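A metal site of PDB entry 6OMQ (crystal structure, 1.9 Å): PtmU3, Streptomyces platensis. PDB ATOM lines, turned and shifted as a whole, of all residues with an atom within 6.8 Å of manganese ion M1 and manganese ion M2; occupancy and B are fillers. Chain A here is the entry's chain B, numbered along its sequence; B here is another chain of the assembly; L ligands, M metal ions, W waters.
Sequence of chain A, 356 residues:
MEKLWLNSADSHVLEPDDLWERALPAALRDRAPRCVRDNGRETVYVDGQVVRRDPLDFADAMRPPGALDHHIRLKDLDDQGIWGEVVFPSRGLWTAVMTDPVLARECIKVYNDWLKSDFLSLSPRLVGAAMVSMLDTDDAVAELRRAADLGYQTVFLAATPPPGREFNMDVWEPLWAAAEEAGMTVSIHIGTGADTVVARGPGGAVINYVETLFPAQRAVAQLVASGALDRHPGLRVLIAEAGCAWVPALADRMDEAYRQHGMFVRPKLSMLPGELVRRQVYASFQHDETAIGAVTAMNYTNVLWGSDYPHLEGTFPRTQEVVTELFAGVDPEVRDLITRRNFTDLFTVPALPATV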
ATOM      1  N   ASP A  10      24.256  -1.414  -4.363  1.00  0.00           N
ATOM      2  CA  ASP A  10      23.277  -0.454  -3.748  1.00  0.00           C
ATOM      3  C   ASP A  10      22.409   0.198  -4.808  1.00  0.00           C
ATOM      4  O   ASP A  10      22.908   0.952  -5.653  1.00  0.00           O
ATOM      5  CB  ASP A  10      24.017   0.628  -2.924  1.00  0.00           C
ATOM      6  CG  ASP A  10      23.254   1.695  -2.150  1.00  0.00           C
ATOM      7  OD1 ASP A  10      22.005   1.620  -1.825  1.00  0.00           O
ATOM      8  OD2 ASP A  10      23.930   2.684  -1.800  1.00  0.00           O
ATOM      9  N   SER A  11      21.080   0.095  -4.605  1.00  0.00           N
ATOM     10  CA  SER A  11      20.057   0.847  -5.349  1.00  0.00           C
ATOM     11  C   SER A  11      18.748   0.694  -4.558  1.00  0.00           C
ATOM     12  O   SER A  11      18.724  -0.154  -3.654  1.00  0.00           O
ATOM     13  CB  SER A  11      19.859   0.325  -6.771  1.00  0.00           C
ATOM     14  OG  SER A  11      19.258  -0.973  -6.693  1.00  0.00           O
ATOM     15  N   HIS A  12      17.745   1.448  -4.976  1.00  0.00           N
ATOM     16  CA  HIS A  12      16.440   1.565  -4.280  1.00  0.00           C
ATOM     17  C   HIS A  12      15.289   1.369  -5.279  1.00  0.00           C
ATOM     18  O   HIS A  12      15.438   1.849  -6.455  1.00  0.00           O
ATOM     19  CB  HIS A  12      16.373   2.912  -3.555  1.00  0.00           C
ATOM     20  CG  HIS A  12      17.437   3.015  -2.500  1.00  0.00           C
ATOM     21  ND1 HIS A  12      17.240   2.517  -1.215  1.00  0.00           N
ATOM     22  CD2 HIS A  12      18.745   3.425  -2.579  1.00  0.00           C
ATOM     23  CE1 HIS A  12      18.406   2.664  -0.520  1.00  0.00           C
ATOM     24  NE2 HIS A  12      19.307   3.248  -1.337  1.00  0.00           N
ATOM     25  N   MET A  62      14.628  11.972  -7.138  1.00  0.00           N
ATOM     26  CA  MET A  62      14.945  10.548  -6.862  1.00  0.00           C
ATOM     27  C   MET A  62      13.979   9.609  -7.573  1.00  0.00           C
ATOM     28  O   MET A  62      14.033   8.396  -7.287  1.00  0.00           O
ATOM     29  CB  MET A  62      14.900  10.280  -5.352  1.00  0.00           C
ATOM     30  CG  MET A  62      15.995  10.998  -4.598  1.00  0.00           C
ATOM     31  SD  MET A  62      15.933  10.571  -2.802  1.00  0.00           S
ATOM     32  CE  MET A  62      14.852  11.871  -2.201  1.00  0.00           C
ATOM     33  N   PHE A  88      17.259  -2.096  -2.443  1.00  0.00           N
ATOM     34  CA  PHE A  88      16.849  -1.752  -1.073  1.00  0.00           C
ATOM     35  C   PHE A  88      15.498  -1.056  -1.150  1.00  0.00           C
ATOM     36  O   PHE A  88      15.111  -0.531  -2.184  1.00  0.00           O
ATOM     37  CB  PHE A  88      17.898  -0.862  -0.390  1.00  0.00           C
ATOM     38  CG  PHE A  88      19.131  -1.621  -0.005  1.00  0.00           C
ATOM     39  CD1 PHE A  88      19.130  -2.443   1.112  1.00  0.00           C
ATOM     40  CD2 PHE A  88      20.292  -1.533  -0.765  1.00  0.00           C
ATOM     41  CE1 PHE A  88      20.256  -3.164   1.479  1.00  0.00           C
ATOM     42  CE2 PHE A  88      21.433  -2.228  -0.391  1.00  0.00           C
ATOM     43  CZ  PHE A  88      21.407  -3.058   0.712  1.00  0.00           C
ATOM     44  N   HIS A 189      21.987  -0.525   5.854  1.00  0.00           N
ATOM     45  CA  HIS A 189      21.980   0.627   4.954  1.00  0.00           C
ATOM     46  C   HIS A 189      21.953   1.848   5.831  1.00  0.00           C
ATOM     47  O   HIS A 189      21.100   1.947   6.720  1.00  0.00           O
ATOM     48  CB  HIS A 189      20.853   0.557   3.916  1.00  0.00           C
ATOM     49  CG  HIS A 189      21.031   1.551   2.831  1.00  0.00           C
ATOM     50  ND1 HIS A 189      20.906   2.884   3.072  1.00  0.00           N
ATOM     51  CD2 HIS A 189      21.289   1.404   1.515  1.00  0.00           C
ATOM     52  CE1 HIS A 189      21.099   3.558   1.940  1.00  0.00           C
ATOM     53  NE2 HIS A 189      21.365   2.662   0.952  1.00  0.00           N
ATOM     54  N   ILE A 190      22.862   2.767   5.567  1.00  0.00           N
ATOM     55  CA  ILE A 190      22.945   3.959   6.440  1.00  0.00           C
ATOM     56  C   ILE A 190      21.749   4.876   6.204  1.00  0.00           C
ATOM     57  O   ILE A 190      20.925   4.647   5.228  1.00  0.00           O
ATOM     58  CB  ILE A 190      24.313   4.667   6.327  1.00  0.00           C
ATOM     59  CG1 ILE A 190      24.643   5.148   4.921  1.00  0.00           C
ATOM     60  CG2 ILE A 190      25.378   3.733   6.854  1.00  0.00           C
ATOM     61  CD1 ILE A 190      23.700   6.177   4.347  1.00  0.00           C
ATOM     62  N   TYR A 209      25.247  14.598   5.817  1.00  0.00           N
ATOM     63  CA  TYR A 209      25.697  13.451   4.991  1.00  0.00           C
ATOM     64  C   TYR A 209      26.825  12.753   5.781  1.00  0.00           C
ATOM     65  O   TYR A 209      26.855  11.545   5.791  1.00  0.00           O
ATOM     66  CB  TYR A 209      26.003  13.873   3.552  1.00  0.00           C
ATOM     67  CG  TYR A 209      26.103  12.715   2.580  1.00  0.00           C
ATOM     68  CD1 TYR A 209      25.060  11.826   2.393  1.00  0.00           C
ATOM     69  CD2 TYR A 209      27.276  12.480   1.860  1.00  0.00           C
ATOM     70  CE1 TYR A 209      25.156  10.743   1.538  1.00  0.00           C
ATOM     71  CE2 TYR A 209      27.354  11.439   0.936  1.00  0.00           C
ATOM     72  CZ  TYR A 209      26.301  10.547   0.767  1.00  0.00           C
ATOM     73  OH  TYR A 209      26.377   9.445  -0.044  1.00  0.00           O
ATOM     74  N   ALA A 240      26.052  -0.515   3.536  1.00  0.00           N
ATOM     75  CA  ALA A 240      25.696   0.039   2.223  1.00  0.00           C
ATOM     76  C   ALA A 240      25.648   1.540   2.342  1.00  0.00           C
ATOM     77  O   ALA A 240      25.053   2.062   3.280  1.00  0.00           O
ATOM     78  CB  ALA A 240      24.381  -0.586   1.749  1.00  0.00           C
ATOM     79  N   GLU A 241      26.322   2.212   1.417  1.00  0.00           N
ATOM     80  CA  GLU A 241      26.233   3.647   1.135  1.00  0.00           C
ATOM     81  C   GLU A 241      26.947   4.463   2.219  1.00  0.00           C
ATOM     82  O   GLU A 241      26.572   5.600   2.414  1.00  0.00           O
ATOM     83  CB  GLU A 241      24.761   4.107   1.036  1.00  0.00           C
ATOM     84  CG  GLU A 241      24.617   5.307   0.139  1.00  0.00           C
ATOM     85  CD  GLU A 241      23.226   5.888  -0.046  1.00  0.00           C
ATOM     86  OE1 GLU A 241      22.259   5.140  -0.392  1.00  0.00           O
ATOM     87  OE2 GLU A 241      23.156   7.147   0.080  1.00  0.00           O
ATOM     88  N   SER A 284      30.111  -0.441   0.619  1.00  0.00           N
ATOM     89  CA  SER A 284      29.883   0.055  -0.750  1.00  0.00           C
ATOM     90  C   SER A 284      30.125   1.534  -0.793  1.00  0.00           C
ATOM     91  O   SER A 284      30.003   2.199   0.245  1.00  0.00           O
ATOM     92  CB  SER A 284      28.457  -0.330  -1.192  1.00  0.00           C
ATOM     93  OG  SER A 284      27.542   0.643  -0.756  1.00  0.00           O
ATOM     94  N   GLN A 286      29.900   4.948  -4.094  1.00  0.00           N
ATOM     95  CA  GLN A 286      29.536   5.406  -5.446  1.00  0.00           C
ATOM     96  C   GLN A 286      30.692   6.127  -6.147  1.00  0.00           C
ATOM     97  O   GLN A 286      31.004   5.750  -7.266  1.00  0.00           O
ATOM     98  CB  GLN A 286      28.330   6.324  -5.321  1.00  0.00           C
ATOM     99  CG  GLN A 286      27.198   5.665  -4.556  1.00  0.00           C
ATOM    100  CD  GLN A 286      27.151   5.972  -3.077  1.00  0.00           C
ATOM    101  OE1 GLN A 286      27.299   5.093  -2.257  1.00  0.00           O
ATOM    102  NE2 GLN A 286      26.886   7.226  -2.756  1.00  0.00           N
ATOM    103  N   ASP A 308      23.863   3.402  -6.243  1.00  0.00           N
ATOM    104  CA  ASP A 308      22.770   3.960  -5.397  1.00  0.00           C
ATOM    105  C   ASP A 308      21.634   4.536  -6.263  1.00  0.00           C
ATOM    106  O   ASP A 308      21.226   5.723  -6.037  1.00  0.00           O
ATOM    107  CB  ASP A 308      23.254   5.082  -4.492  1.00  0.00           C
ATOM    108  CG  ASP A 308      22.279   5.337  -3.359  1.00  0.00           C
ATOM    109  OD1 ASP A 308      21.643   4.368  -2.867  1.00  0.00           O
ATOM    110  OD2 ASP A 308      22.277   6.429  -2.922  1.00  0.00           O
ATOM    111  N   TYR A 309      21.373   3.865  -7.371  1.00  0.00           N
ATOM    112  CA  TYR A 309      20.271   4.262  -8.317  1.00  0.00           C
ATOM    113  C   TYR A 309      18.988   4.316  -7.480  1.00  0.00           C
ATOM    114  O   TYR A 309      18.700   3.325  -6.823  1.00  0.00           O
ATOM    115  CB  TYR A 309      20.135   3.212  -9.404  1.00  0.00           C
ATOM    116  CG  TYR A 309      18.980   3.451 -10.353  1.00  0.00           C
ATOM    117  CD1 TYR A 309      19.125   4.257 -11.470  1.00  0.00           C
ATOM    118  CD2 TYR A 309      17.726   2.881 -10.119  1.00  0.00           C
ATOM    119  CE1 TYR A 309      18.082   4.472 -12.361  1.00  0.00           C
ATOM    120  CE2 TYR A 309      16.664   3.098 -10.993  1.00  0.00           C
ATOM    121  CZ  TYR A 309      16.833   3.899 -12.113  1.00  0.00           C
ATOM    122  OH  TYR A 309      15.811   4.112 -12.997  1.00  0.00           O
ATOM    123  N   HIS A 311      19.241   7.749  -6.366  1.00  0.00           N
ATOM    124  CA  HIS A 311      19.481   8.859  -5.449  1.00  0.00           C
ATOM    125  C   HIS A 311      20.467   9.826  -6.092  1.00  0.00           C
ATOM    126  O   HIS A 311      21.264   9.394  -6.893  1.00  0.00           O
ATOM    127  CB  HIS A 311      19.962   8.308  -4.093  1.00  0.00           C
ATOM    128  CG  HIS A 311      18.908   7.541  -3.374  1.00  0.00           C
ATOM    129  ND1 HIS A 311      19.067   7.102  -2.051  1.00  0.00           N
ATOM    130  CD2 HIS A 311      17.648   7.166  -3.774  1.00  0.00           C
ATOM    131  CE1 HIS A 311      17.969   6.496  -1.678  1.00  0.00           C
ATOM    132  NE2 HIS A 311      17.079   6.504  -2.726  1.00  0.00           N
ATOM    133  N   LEU A 312      20.416  11.072  -5.689  1.00  0.00           N
ATOM    134  CA  LEU A 312      21.336  12.115  -6.135  1.00  0.00           C
ATOM    135  C   LEU A 312      22.777  11.736  -5.767  1.00  0.00           C
ATOM    136  O   LEU A 312      23.654  12.161  -6.482  1.00  0.00           O
ATOM    137  CB  LEU A 312      20.932  13.413  -5.446  1.00  0.00           C
ATOM    138  CG  LEU A 312      19.788  14.159  -6.103  1.00  0.00           C
ATOM    139  CD1 LEU A 312      18.626  13.224  -6.375  1.00  0.00           C
ATOM    140  CD2 LEU A 312      19.373  15.333  -5.232  1.00  0.00           C
ATOM    141  N   GLU A 313      22.975  10.994  -4.660  1.00  0.00           N
ATOM    142  CA  GLU A 313      24.304  10.625  -4.089  1.00  0.00           C
ATOM    143  C   GLU A 313      24.969   9.658  -5.067  1.00  0.00           C
ATOM    144  O   GLU A 313      26.155   9.369  -4.879  1.00  0.00           O
ATOM    145  CB  GLU A 313      24.285   9.703  -2.852  1.00  0.00           C
ATOM    146  CG  GLU A 313      23.470  10.021  -1.671  1.00  0.00           C
ATOM    147  CD  GLU A 313      21.962   9.922  -1.743  1.00  0.00           C
ATOM    148  OE1 GLU A 313      21.321   8.833  -1.412  1.00  0.00           O
ATOM    149  OE2 GLU A 313      21.463  10.948  -2.141  1.00  0.00           O
ATOM    150  N   GLY A 314      24.159   9.015  -5.914  1.00  0.00           N
ATOM    151  CA  GLY A 314      24.602   7.930  -6.802  1.00  0.00           C
ATOM    152  C   GLY A 314      25.134   8.445  -8.151  1.00  0.00           C
ATOM    153  O   GLY A 314      25.266   9.612  -8.320  1.00  0.00           O
ATOM    154  N   HIS B 261      24.360  17.111  -3.680  1.00  0.00           N
ATOM    155  CA  HIS B 261      23.280  17.672  -2.831  1.00  0.00           C
ATOM    156  C   HIS B 261      23.415  19.191  -2.861  1.00  0.00           C
ATOM    157  O   HIS B 261      22.880  19.840  -1.953  1.00  0.00           O
ATOM    158  CB  HIS B 261      23.298  17.136  -1.369  1.00  0.00           C
ATOM    159  CG  HIS B 261      22.956  15.701  -1.183  1.00  0.00           C
ATOM    160  ND1 HIS B 261      22.980  15.107   0.071  1.00  0.00           N
ATOM    161  CD2 HIS B 261      22.626  14.720  -2.053  1.00  0.00           C
ATOM    162  CE1 HIS B 261      22.671  13.832  -0.036  1.00  0.00           C
ATOM    163  NE2 HIS B 261      22.442  13.564  -1.333  1.00  0.00           N
HETATM  164  C1  LIG L   1      14.983   7.469   2.658  1.00  0.00           C
HETATM  165  C2  LIG L   1      18.269   8.837   4.224  1.00  0.00           C
HETATM  166  C3  LIG L   1      20.361   9.824   3.008  1.00  0.00           C
HETATM  167  C4  LIG L   1      20.462  10.970   4.060  1.00  0.00           C
HETATM  168  C5  LIG L   1      20.122  14.142   5.138  1.00  0.00           C
HETATM  169  C6  LIG L   1      19.018  15.614   3.561  1.00  0.00           C
HETATM  170  C7  LIG L   1      20.025  17.746   2.677  1.00  0.00           C
HETATM  171  C8  LIG L   1      19.520  18.769   4.906  1.00  0.00           C
HETATM  172  O1  LIG L   1      17.029  24.699   6.266  1.00  0.00           O
HETATM  173  P1  LIG L   1      17.538  24.360   7.614  1.00  0.00           P
HETATM  174  O2  LIG L   1      16.637  23.652   8.562  1.00  0.00           O
HETATM  175  O3  LIG L   1      18.647  25.185   8.181  1.00  0.00           O
HETATM  176  O4  LIG L   1      18.491  23.075   7.145  1.00  0.00           O
HETATM  177  C9  LIG L   1      17.960  21.914   6.539  1.00  0.00           C
HETATM  178  C10 LIG L   1      19.130  21.103   5.945  1.00  0.00           C
HETATM  179  C11 LIG L   1      19.621  21.748   4.624  1.00  0.00           C
HETATM  180  C12 LIG L   1      20.307  21.049   6.945  1.00  0.00           C
HETATM  181  C13 LIG L   1      18.542  19.680   5.674  1.00  0.00           C
HETATM  182  O5  LIG L   1      17.316  19.813   4.897  1.00  0.00           O
HETATM  183  O6  LIG L   1      20.503  18.300   5.475  1.00  0.00           O
HETATM  184  N1  LIG L   1      19.226  18.592   3.577  1.00  0.00           N
HETATM  185  C14 LIG L   1      19.100  16.577   2.330  1.00  0.00           C
HETATM  186  O7  LIG L   1      17.957  15.444   4.178  1.00  0.00           O
HETATM  187  N2  LIG L   1      20.161  15.096   4.016  1.00  0.00           N
HETATM  188  C15 LIG L   1      21.468  13.393   5.122  1.00  0.00           C
HETATM  189  S1  LIG L   1      21.568  12.323   3.600  1.00  0.00           S
HETATM  190  O8  LIG L   1      19.879  10.933   5.145  1.00  0.00           O
HETATM  191  C16 LIG L   1      21.278   8.685   3.509  1.00  0.00           C
HETATM  192  C17 LIG L   1      20.918  10.235   1.652  1.00  0.00           C
HETATM  193  C18 LIG L   1      19.912  11.119   0.865  1.00  0.00           C
HETATM  194  C19 LIG L   1      18.604  10.392   0.678  1.00  0.00           C
HETATM  195  C20 LIG L   1      17.866  10.171   2.062  1.00  0.00           C
HETATM  196  C21 LIG L   1      17.515  11.507   2.776  1.00  0.00           C
HETATM  197  C22 LIG L   1      16.581   9.249   1.795  1.00  0.00           C
HETATM  198  C23 LIG L   1      18.844   9.249   2.883  1.00  0.00           C
HETATM  199  C24 LIG L   1      17.042   7.901   3.978  1.00  0.00           C
HETATM  200  O9  LIG L   1      16.376   7.610   5.272  1.00  0.00           O
HETATM  201  C25 LIG L   1      15.993   8.562   3.102  1.00  0.00           C
HETATM  202  C26 LIG L   1      13.974   8.293   1.876  1.00  0.00           C
HETATM  203  C27 LIG L   1      12.670   7.520   1.756  1.00  0.00           C
HETATM  204  O10 LIG L   1      14.516   8.728   0.530  1.00  0.00           O
HETATM  205  C28 LIG L   1      15.390   9.840   0.932  1.00  0.00           C
HETATM  206  C29 LIG L   1      14.401  10.686   1.716  1.00  0.00           C
HETATM  207  C30 LIG L   1      13.944   9.624   2.722  1.00  0.00           C
HETATM  208  C31 LIG L   1      15.009   9.462   3.840  1.00  0.00           C
HETATM  209 MN    MN M   1      21.549   3.371  -1.125  1.00  0.00          MN
HETATM  210 MN    MN M   2      21.260   7.114  -1.103  1.00  0.00          MN
HETATM  211  O   HOH W   1      19.916   6.652   0.923  1.00  0.00           O
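Manganese ion M1 is bound by the side-chain carboxylate (OD1) of Asp 10, the side-chain carboxylate (OD1) of Asp 308, the side-chain carboxylate (OE1) of Glu 241, a ring nitrogen (NE2) of His 189, a ring nitrogen (NE2) of His 12 and the side-chain carboxylate (OD2) of Asp 10. Manganese ion M1 has six donor atoms within binding distance.
O of Glu 313 sits at hydrogen-bond distance from NE2 of Gln 286, 3.1 Å away. A ring nitrogen (NE2) of His 261 of chain B sits at hydrogen-bond distance from the side-chain carboxylate (OE2) of Glu 313 (2.9 Å). The side-chain hydroxyl (OG) of Ser 284 lies within hydrogen-bond range of the backbone NH (N) of Glu 241 (2.9 Å). The backbone NH (N) of His 12 lies within hydrogen-bond range of the backbone carbonyl oxygen (O) of Tyr 309, at 2.8 Å.
Of the 19 residues printed, 5 come within 4 Å of manganese ion M1.
Manganese ion M2 is bound by the side-chain carboxylate (OE1) of Glu 313 (1.7 Å), the side-chain carboxylate (OD2) of Asp 308 (2.2 Å), the side-chain carboxylate (OE2) of Glu 241 (2.2 Å), the side-chain carboxylate (OE1) of Glu 241 (2.3 Å), a ring nitrogen (ND1) of His 311 (2.4 Å) and water W1 (2.5 Å).
The nearest printed residue that does not touch manganese ion M2 is His 12 (4.3 Å).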
